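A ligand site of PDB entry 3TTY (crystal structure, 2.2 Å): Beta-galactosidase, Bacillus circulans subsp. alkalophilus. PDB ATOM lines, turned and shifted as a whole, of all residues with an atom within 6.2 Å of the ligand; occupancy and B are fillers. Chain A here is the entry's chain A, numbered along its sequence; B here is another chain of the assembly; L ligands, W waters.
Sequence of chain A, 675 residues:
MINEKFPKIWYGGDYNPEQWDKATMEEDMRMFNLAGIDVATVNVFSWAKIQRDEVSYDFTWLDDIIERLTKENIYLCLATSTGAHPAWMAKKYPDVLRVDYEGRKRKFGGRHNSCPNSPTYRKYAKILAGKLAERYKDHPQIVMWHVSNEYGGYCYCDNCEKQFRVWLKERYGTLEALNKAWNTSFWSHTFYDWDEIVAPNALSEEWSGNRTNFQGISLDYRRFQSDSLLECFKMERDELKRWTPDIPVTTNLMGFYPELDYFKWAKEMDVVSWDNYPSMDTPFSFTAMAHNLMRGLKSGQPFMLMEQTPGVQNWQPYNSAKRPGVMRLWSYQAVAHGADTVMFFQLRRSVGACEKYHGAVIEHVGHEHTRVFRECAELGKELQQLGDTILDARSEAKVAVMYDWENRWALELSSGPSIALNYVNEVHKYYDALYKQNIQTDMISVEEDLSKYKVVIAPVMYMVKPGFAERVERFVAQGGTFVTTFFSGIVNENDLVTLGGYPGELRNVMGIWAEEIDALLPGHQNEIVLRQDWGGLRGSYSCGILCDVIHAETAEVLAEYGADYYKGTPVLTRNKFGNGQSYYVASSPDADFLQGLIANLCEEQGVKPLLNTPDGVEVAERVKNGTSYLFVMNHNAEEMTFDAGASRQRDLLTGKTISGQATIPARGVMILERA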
ATOM      1  N   ASP A  14     -11.769   2.264 -23.089  1.00  0.00           N
ATOM      2  CA  ASP A  14     -12.810   2.483 -22.094  1.00  0.00           C
ATOM      3  C   ASP A  14     -13.358   3.907 -22.198  1.00  0.00           C
ATOM      4  O   ASP A  14     -12.606   4.875 -22.237  1.00  0.00           O
ATOM      5  CB  ASP A  14     -12.283   2.215 -20.686  1.00  0.00           C
ATOM      6  CG  ASP A  14     -12.338   0.729 -20.288  1.00  0.00           C
ATOM      7  OD1 ASP A  14     -11.923  -0.135 -21.090  1.00  0.00           O
ATOM      8  OD2 ASP A  14     -12.789   0.422 -19.160  1.00  0.00           O
ATOM      9  N   VAL A  44     -18.933  -0.652 -18.746  1.00  0.00           N
ATOM     10  CA  VAL A  44     -18.147  -1.565 -17.895  1.00  0.00           C
ATOM     11  C   VAL A  44     -18.622  -1.483 -16.438  1.00  0.00           C
ATOM     12  O   VAL A  44     -18.638  -2.490 -15.736  1.00  0.00           O
ATOM     13  CB  VAL A  44     -16.642  -1.281 -17.952  1.00  0.00           C
ATOM     14  CG1 VAL A  44     -15.877  -2.273 -17.085  1.00  0.00           C
ATOM     15  CG2 VAL A  44     -16.134  -1.327 -19.372  1.00  0.00           C
ATOM     16  N   PHE A  45     -19.033  -0.305 -16.004  1.00  0.00           N
ATOM     17  CA  PHE A  45     -19.287  -0.091 -14.585  1.00  0.00           C
ATOM     18  C   PHE A  45     -20.596   0.624 -14.302  1.00  0.00           C
ATOM     19  O   PHE A  45     -20.612   1.653 -13.625  1.00  0.00           O
ATOM     20  CB  PHE A  45     -18.126   0.667 -13.934  1.00  0.00           C
ATOM     21  CG  PHE A  45     -16.875  -0.171 -13.752  1.00  0.00           C
ATOM     22  CD1 PHE A  45     -16.887  -1.287 -12.929  1.00  0.00           C
ATOM     23  CD2 PHE A  45     -15.691   0.168 -14.372  1.00  0.00           C
ATOM     24  CE1 PHE A  45     -15.737  -2.066 -12.735  1.00  0.00           C
ATOM     25  CE2 PHE A  45     -14.532  -0.596 -14.192  1.00  0.00           C
ATOM     26  CZ  PHE A  45     -14.567  -1.714 -13.378  1.00  0.00           C
ATOM     27  N   ARG A 111     -14.504  -3.014  -6.119  1.00  0.00           N
ATOM     28  CA  ARG A 111     -15.016  -3.648  -7.327  1.00  0.00           C
ATOM     29  C   ARG A 111     -14.357  -5.029  -7.469  1.00  0.00           C
ATOM     30  O   ARG A 111     -13.513  -5.390  -6.645  1.00  0.00           O
ATOM     31  CB  ARG A 111     -14.686  -2.783  -8.532  1.00  0.00           C
ATOM     32  CG  ARG A 111     -13.196  -2.520  -8.674  1.00  0.00           C
ATOM     33  CD  ARG A 111     -12.829  -2.016 -10.059  1.00  0.00           C
ATOM     34  NE  ARG A 111     -11.377  -1.880 -10.213  1.00  0.00           N
ATOM     35  CZ  ARG A 111     -10.780  -1.355 -11.279  1.00  0.00           C
ATOM     36  NH1 ARG A 111     -11.499  -0.913 -12.300  1.00  0.00           N
ATOM     37  NH2 ARG A 111      -9.449  -1.296 -11.322  1.00  0.00           N
ATOM     38  N   HIS A 112     -14.730  -5.772  -8.517  1.00  0.00           N
ATOM     39  CA  HIS A 112     -14.089  -7.050  -8.861  1.00  0.00           C
ATOM     40  C   HIS A 112     -14.091  -8.048  -7.708  1.00  0.00           C
ATOM     41  O   HIS A 112     -13.214  -8.905  -7.628  1.00  0.00           O
ATOM     42  CB  HIS A 112     -12.614  -6.863  -9.258  1.00  0.00           C
ATOM     43  CG  HIS A 112     -12.413  -5.900 -10.384  1.00  0.00           C
ATOM     44  ND1 HIS A 112     -11.177  -5.334 -10.655  1.00  0.00           N
ATOM     45  CD2 HIS A 112     -13.262  -5.378 -11.290  1.00  0.00           C
ATOM     46  CE1 HIS A 112     -11.283  -4.534 -11.694  1.00  0.00           C
ATOM     47  NE2 HIS A 112     -12.540  -4.527 -12.097  1.00  0.00           N
ATOM     48  N   ASN A 149     -15.199  -7.464 -15.706  1.00  0.00           N
ATOM     49  CA  ASN A 149     -13.960  -6.702 -15.817  1.00  0.00           C
ATOM     50  C   ASN A 149     -12.937  -7.278 -14.844  1.00  0.00           C
ATOM     51  O   ASN A 149     -13.232  -7.454 -13.656  1.00  0.00           O
ATOM     52  CB  ASN A 149     -14.186  -5.229 -15.521  1.00  0.00           C
ATOM     53  CG  ASN A 149     -12.992  -4.377 -15.900  1.00  0.00           C
ATOM     54  OD1 ASN A 149     -12.657  -4.258 -17.073  1.00  0.00           O
ATOM     55  ND2 ASN A 149     -12.328  -3.788 -14.907  1.00  0.00           N
ATOM     56  N   GLU A 150     -11.735  -7.551 -15.353  1.00  0.00           N
ATOM     57  CA  GLU A 150     -10.643  -8.121 -14.551  1.00  0.00           C
ATOM     58  C   GLU A 150     -11.101  -9.042 -13.386  1.00  0.00           C
ATOM     59  O   GLU A 150     -10.972  -8.688 -12.215  1.00  0.00           O
ATOM     60  CB  GLU A 150      -9.705  -7.019 -14.019  1.00  0.00           C
ATOM     61  CG  GLU A 150      -8.995  -6.221 -15.096  1.00  0.00           C
ATOM     62  CD  GLU A 150      -7.777  -5.458 -14.567  1.00  0.00           C
ATOM     63  OE1 GLU A 150      -7.726  -5.132 -13.354  1.00  0.00           O
ATOM     64  OE2 GLU A 150      -6.846  -5.207 -15.376  1.00  0.00           O
ATOM     65  N   ASN A 252     -11.136  -9.239 -19.808  1.00  0.00           N
ATOM     66  CA  ASN A 252      -9.788  -8.660 -19.844  1.00  0.00           C
ATOM     67  C   ASN A 252      -8.846  -9.198 -18.755  1.00  0.00           C
ATOM     68  O   ASN A 252      -9.136  -9.102 -17.555  1.00  0.00           O
ATOM     69  CB  ASN A 252      -9.826  -7.110 -19.866  1.00  0.00           C
ATOM     70  CG  ASN A 252     -10.695  -6.511 -18.766  1.00  0.00           C
ATOM     71  OD1 ASN A 252     -11.526  -7.199 -18.182  1.00  0.00           O
ATOM     72  ND2 ASN A 252     -10.519  -5.230 -18.502  1.00  0.00           N
ATOM     73  N   ASP A 275      -4.540  -6.096 -20.194  1.00  0.00           N
ATOM     74  CA  ASP A 275      -4.366  -4.724 -19.765  1.00  0.00           C
ATOM     75  C   ASP A 275      -2.905  -4.513 -19.380  1.00  0.00           C
ATOM     76  O   ASP A 275      -2.430  -5.014 -18.371  1.00  0.00           O
ATOM     77  CB  ASP A 275      -5.297  -4.439 -18.575  1.00  0.00           C
ATOM     78  CG  ASP A 275      -6.780  -4.792 -18.883  1.00  0.00           C
ATOM     79  OD1 ASP A 275      -7.189  -4.762 -20.062  1.00  0.00           O
ATOM     80  OD2 ASP A 275      -7.541  -5.090 -17.929  1.00  0.00           O
ATOM     81  N   TYR A 277       0.148  -2.337 -18.181  1.00  0.00           N
ATOM     82  CA  TYR A 277       0.535  -1.157 -17.400  1.00  0.00           C
ATOM     83  C   TYR A 277       1.953  -1.263 -16.858  1.00  0.00           C
ATOM     84  O   TYR A 277       2.157  -1.574 -15.694  1.00  0.00           O
ATOM     85  CB  TYR A 277      -0.449  -0.944 -16.255  1.00  0.00           C
ATOM     86  CG  TYR A 277      -1.837  -0.546 -16.733  1.00  0.00           C
ATOM     87  CD1 TYR A 277      -2.149   0.786 -16.967  1.00  0.00           C
ATOM     88  CD2 TYR A 277      -2.811  -1.503 -16.970  1.00  0.00           C
ATOM     89  CE1 TYR A 277      -3.409   1.157 -17.413  1.00  0.00           C
ATOM     90  CE2 TYR A 277      -4.072  -1.144 -17.409  1.00  0.00           C
ATOM     91  CZ  TYR A 277      -4.362   0.191 -17.633  1.00  0.00           C
ATOM     92  OH  TYR A 277      -5.617   0.552 -18.079  1.00  0.00           O
ATOM     93  N   GLU A 307      -6.435  -2.581 -22.709  1.00  0.00           N
ATOM     94  CA  GLU A 307      -6.046  -1.345 -22.039  1.00  0.00           C
ATOM     95  C   GLU A 307      -4.542  -1.111 -21.935  1.00  0.00           C
ATOM     96  O   GLU A 307      -3.722  -2.031 -22.008  1.00  0.00           O
ATOM     97  CB  GLU A 307      -6.613  -1.253 -20.629  1.00  0.00           C
ATOM     98  CG  GLU A 307      -8.073  -1.575 -20.450  1.00  0.00           C
ATOM     99  CD  GLU A 307      -8.404  -1.700 -18.984  1.00  0.00           C
ATOM    100  OE1 GLU A 307      -7.698  -1.043 -18.190  1.00  0.00           O
ATOM    101  OE2 GLU A 307      -9.344  -2.453 -18.609  1.00  0.00           O
ATOM    102  N   GLN A 313      -0.387   6.402 -14.837  1.00  0.00           N
ATOM    103  CA  GLN A 313      -1.318   5.506 -14.166  1.00  0.00           C
ATOM    104  C   GLN A 313      -1.303   5.826 -12.671  1.00  0.00           C
ATOM    105  O   GLN A 313      -0.257   5.823 -12.031  1.00  0.00           O
ATOM    106  CB  GLN A 313      -0.960   4.036 -14.397  1.00  0.00           C
ATOM    107  CG  GLN A 313      -1.930   3.044 -13.675  1.00  0.00           C
ATOM    108  CD  GLN A 313      -1.402   1.611 -13.645  1.00  0.00           C
ATOM    109  OE1 GLN A 313      -2.174   0.651 -13.543  1.00  0.00           O
ATOM    110  NE2 GLN A 313      -0.087   1.466 -13.755  1.00  0.00           N
ATOM    111  N   ASN A 314      -2.475   6.122 -12.118  1.00  0.00           N
ATOM    112  CA  ASN A 314      -2.580   6.554 -10.744  1.00  0.00           C
ATOM    113  C   ASN A 314      -2.098   5.497  -9.765  1.00  0.00           C
ATOM    114  O   ASN A 314      -1.577   5.828  -8.708  1.00  0.00           O
ATOM    115  CB  ASN A 314      -4.019   6.910 -10.433  1.00  0.00           C
ATOM    116  CG  ASN A 314      -4.945   5.734 -10.602  1.00  0.00           C
ATOM    117  OD1 ASN A 314      -5.178   5.282 -11.715  1.00  0.00           O
ATOM    118  ND2 ASN A 314      -5.485   5.245  -9.502  1.00  0.00           N
ATOM    119  N   TRP A 315      -2.272   4.227 -10.129  1.00  0.00           N
ATOM    120  CA  TRP A 315      -1.943   3.106  -9.235  1.00  0.00           C
ATOM    121  C   TRP A 315      -0.462   2.906  -8.979  1.00  0.00           C
ATOM    122  O   TRP A 315      -0.081   2.290  -8.003  1.00  0.00           O
ATOM    123  CB  TRP A 315      -2.587   1.805  -9.732  1.00  0.00           C
ATOM    124  CG  TRP A 315      -4.090   1.888  -9.805  1.00  0.00           C
ATOM    125  CD1 TRP A 315      -4.851   2.094 -10.938  1.00  0.00           C
ATOM    126  CD2 TRP A 315      -5.006   1.822  -8.706  1.00  0.00           C
ATOM    127  NE1 TRP A 315      -6.188   2.142 -10.589  1.00  0.00           N
ATOM    128  CE2 TRP A 315      -6.304   1.974  -9.237  1.00  0.00           C
ATOM    129  CE3 TRP A 315      -4.851   1.637  -7.335  1.00  0.00           C
ATOM    130  CZ2 TRP A 315      -7.449   1.936  -8.431  1.00  0.00           C
ATOM    131  CZ3 TRP A 315      -5.990   1.602  -6.535  1.00  0.00           C
ATOM    132  CH2 TRP A 315      -7.262   1.755  -7.084  1.00  0.00           C
ATOM    133  N   PHE A 345      -7.238   2.563 -21.331  1.00  0.00           N
ATOM    134  CA  PHE A 345      -8.043   3.157 -20.274  1.00  0.00           C
ATOM    135  C   PHE A 345      -7.463   4.551 -20.032  1.00  0.00           C
ATOM    136  O   PHE A 345      -6.252   4.666 -19.821  1.00  0.00           O
ATOM    137  CB  PHE A 345      -8.011   2.348 -18.978  1.00  0.00           C
ATOM    138  CG  PHE A 345      -8.937   2.897 -17.918  1.00  0.00           C
ATOM    139  CD1 PHE A 345     -10.243   2.432 -17.812  1.00  0.00           C
ATOM    140  CD2 PHE A 345      -8.519   3.897 -17.051  1.00  0.00           C
ATOM    141  CE1 PHE A 345     -11.119   2.938 -16.857  1.00  0.00           C
ATOM    142  CE2 PHE A 345      -9.389   4.420 -16.083  1.00  0.00           C
ATOM    143  CZ  PHE A 345     -10.683   3.937 -15.988  1.00  0.00           C
ATOM    144  N   GLU A 355      -9.569   7.185  -9.552  1.00  0.00           N
ATOM    145  CA  GLU A 355      -8.848   7.188 -10.814  1.00  0.00           C
ATOM    146  C   GLU A 355      -8.757   8.561 -11.522  1.00  0.00           C
ATOM    147  O   GLU A 355      -8.274   8.656 -12.640  1.00  0.00           O
ATOM    148  CB  GLU A 355      -9.359   6.058 -11.734  1.00  0.00           C
ATOM    149  CG  GLU A 355      -8.967   4.665 -11.166  1.00  0.00           C
ATOM    150  CD  GLU A 355      -9.352   3.483 -12.053  1.00  0.00           C
ATOM    151  OE1 GLU A 355      -8.692   2.415 -11.936  1.00  0.00           O
ATOM    152  OE2 GLU A 355     -10.318   3.595 -12.833  1.00  0.00           O
ATOM    153  N   HIS A 358      -5.629   9.090 -13.146  1.00  0.00           N
ATOM    154  CA  HIS A 358      -5.301   8.194 -14.257  1.00  0.00           C
ATOM    155  C   HIS A 358      -5.368   8.968 -15.576  1.00  0.00           C
ATOM    156  O   HIS A 358      -6.278   9.776 -15.793  1.00  0.00           O
ATOM    157  CB  HIS A 358      -6.230   6.976 -14.295  1.00  0.00           C
ATOM    158  CG  HIS A 358      -5.693   5.833 -15.101  1.00  0.00           C
ATOM    159  ND1 HIS A 358      -5.622   5.856 -16.478  1.00  0.00           N
ATOM    160  CD2 HIS A 358      -5.189   4.628 -14.724  1.00  0.00           C
ATOM    161  CE1 HIS A 358      -5.090   4.723 -16.915  1.00  0.00           C
ATOM    162  NE2 HIS A 358      -4.818   3.961 -15.865  1.00  0.00           N
ATOM    163  N   PHE B 186     -18.968   6.332 -11.144  1.00  0.00           N
ATOM    164  CA  PHE B 186     -17.721   5.584 -11.233  1.00  0.00           C
ATOM    165  C   PHE B 186     -17.860   4.284 -10.463  1.00  0.00           C
ATOM    166  O   PHE B 186     -18.404   4.269  -9.358  1.00  0.00           O
ATOM    167  CB  PHE B 186     -16.583   6.415 -10.632  1.00  0.00           C
ATOM    168  CG  PHE B 186     -15.222   5.760 -10.677  1.00  0.00           C
ATOM    169  CD1 PHE B 186     -14.512   5.686 -11.864  1.00  0.00           C
ATOM    170  CD2 PHE B 186     -14.649   5.241  -9.527  1.00  0.00           C
ATOM    171  CE1 PHE B 186     -13.263   5.108 -11.898  1.00  0.00           C
ATOM    172  CE2 PHE B 186     -13.385   4.650  -9.552  1.00  0.00           C
ATOM    173  CZ  PHE B 186     -12.686   4.581 -10.733  1.00  0.00           C
ATOM    174  N   TRP B 187     -17.365   3.193 -11.043  1.00  0.00           N
ATOM    175  CA  TRP B 187     -17.421   1.874 -10.426  1.00  0.00           C
ATOM    176  C   TRP B 187     -18.822   1.539  -9.897  1.00  0.00           C
ATOM    177  O   TRP B 187     -18.951   0.943  -8.842  1.00  0.00           O
ATOM    178  CB  TRP B 187     -16.377   1.747  -9.307  1.00  0.00           C
ATOM    179  CG  TRP B 187     -14.981   1.665  -9.825  1.00  0.00           C
ATOM    180  CD1 TRP B 187     -14.576   1.795 -11.133  1.00  0.00           C
ATOM    181  CD2 TRP B 187     -13.790   1.423  -9.067  1.00  0.00           C
ATOM    182  NE1 TRP B 187     -13.222   1.652 -11.217  1.00  0.00           N
ATOM    183  CE2 TRP B 187     -12.707   1.414  -9.963  1.00  0.00           C
ATOM    184  CE3 TRP B 187     -13.543   1.209  -7.704  1.00  0.00           C
ATOM    185  CZ2 TRP B 187     -11.386   1.225  -9.549  1.00  0.00           C
ATOM    186  CZ3 TRP B 187     -12.235   1.000  -7.297  1.00  0.00           C
ATOM    187  CH2 TRP B 187     -11.175   1.020  -8.219  1.00  0.00           C
HETATM  188  C1  LIG L   1      -7.449  -1.993 -14.926  1.00  0.00           C
HETATM  189  C2  LIG L   1      -8.993  -1.877 -15.013  1.00  0.00           C
HETATM  190  C3  LIG L   1      -9.458  -0.494 -15.525  1.00  0.00           C
HETATM  191  C4  LIG L   1      -8.708   0.569 -14.736  1.00  0.00           C
HETATM  192  C5  LIG L   1      -7.200   0.316 -14.831  1.00  0.00           C
HETATM  193  C6  LIG L   1      -6.480   1.438 -14.092  1.00  0.00           C
HETATM  194  O1  LIG L   1      -6.759  -2.064 -16.179  1.00  0.00           O
HETATM  195  O2  LIG L   1      -9.518  -2.879 -15.871  1.00  0.00           O
HETATM  196  O3  LIG L   1     -10.872  -0.304 -15.344  1.00  0.00           O
HETATM  197  O4  LIG L   1      -9.126   0.426 -13.386  1.00  0.00           O
HETATM  198  O5  LIG L   1      -6.891  -0.917 -14.182  1.00  0.00           O
HETATM  199  O6  LIG L   1      -5.096   1.470 -14.476  1.00  0.00           O
HETATM  200  O   HOH W   1      -4.389  -1.429 -13.584  1.00  0.00           O
HETATM  201  O   HOH W   2      -4.817  -3.967 -14.828  1.00  0.00           O
HETATM  202  O   HOH W   3     -12.019   1.996 -13.926  1.00  0.00           O
HETATM  203  O   HOH W   4     -12.389  -1.388 -17.288  1.00  0.00           O
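The indole nitrogen of Trp 315 lies within hydrogen-bond range of the side-chain carboxylate of Glu 355, 2.9 Å away.
NE of Arg 111 sits close to NE2 of His 112, 3.5 Å away.
ND2 of Asn 252 is in hydrogen-bond range of OD1 of Asn 149, 2.7 Å away.
A ring nitrogen (NE2) of His 112 sits at hydrogen-bond distance from the side-chain amide nitrogen of Asn 149.
OD2 of Asp 275 lies close to OE2 of Glu 150, at 2.6 Å.
The backbone NH (N) of Glu 150 lies within hydrogen-bond range of the side-chain amide oxygen (OD1) of Asn 252 (2.9 Å).
The side-chain carboxylate of Asp 275 sits at hydrogen-bond distance from the side-chain amide nitrogen of Asn 252, 3.0 Å away.
NE1 of Trp 315 sits close to ND2 of Asn 314, at 3.4 Å.
Water W1 lies within hydrogen-bond range of O5 of the ligand (2.6 Å) and OE1 of Gln 313 (3.0 Å).
Water W3 lies within hydrogen-bond range of OE2 of Glu 355, O3 of the ligand, NE1 of Trp 187 of chain B and NH1 of Arg 111.
Water W2 bridges the side-chain carboxylate of Glu 150 and an oxygen (O1) of the ligand.
An oxygen (O1) of the ligand sits at hydrogen-bond distance from the side-chain carboxylate of Glu 307 (2.4 Å).
The side-chain carboxylate (OE1) of Glu 355 sits at hydrogen-bond distance from an oxygen (O4) of the ligand.
The guanidinium group (NH2) of Arg 111 lies within hydrogen-bond range of an oxygen (O4) of the ligand (2.7 Å).
NE2 of His 358 lies within hydrogen-bond range of O6 of the ligand.
The side-chain hydroxyl of Tyr 277 lies close to an oxygen (O1) of the ligand, 3.4 Å away.
O2 of the ligand sits at hydrogen-bond distance from ND2 of Asn 149, 3.1 Å away.
The side-chain amide oxygen (OE1) of Gln 313 sits at hydrogen-bond distance from an oxygen (O6) of the ligand, at 3.2 Å.
OE2 of Glu 150 is in hydrogen-bond range of O1 of the ligand (3.2 Å).
Merely in contact with the ligand: Asp 275, Trp 315, Phe 345, Asn 252 and Phe 45.
Hydrophobic or aromatic side chains within 4 Å of the ligand: Phe 45, Tyr 277, Trp 315, Phe 345 and His 358.
Along chain A the residues within 4 Å of the ligand span positions 45 to 358.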
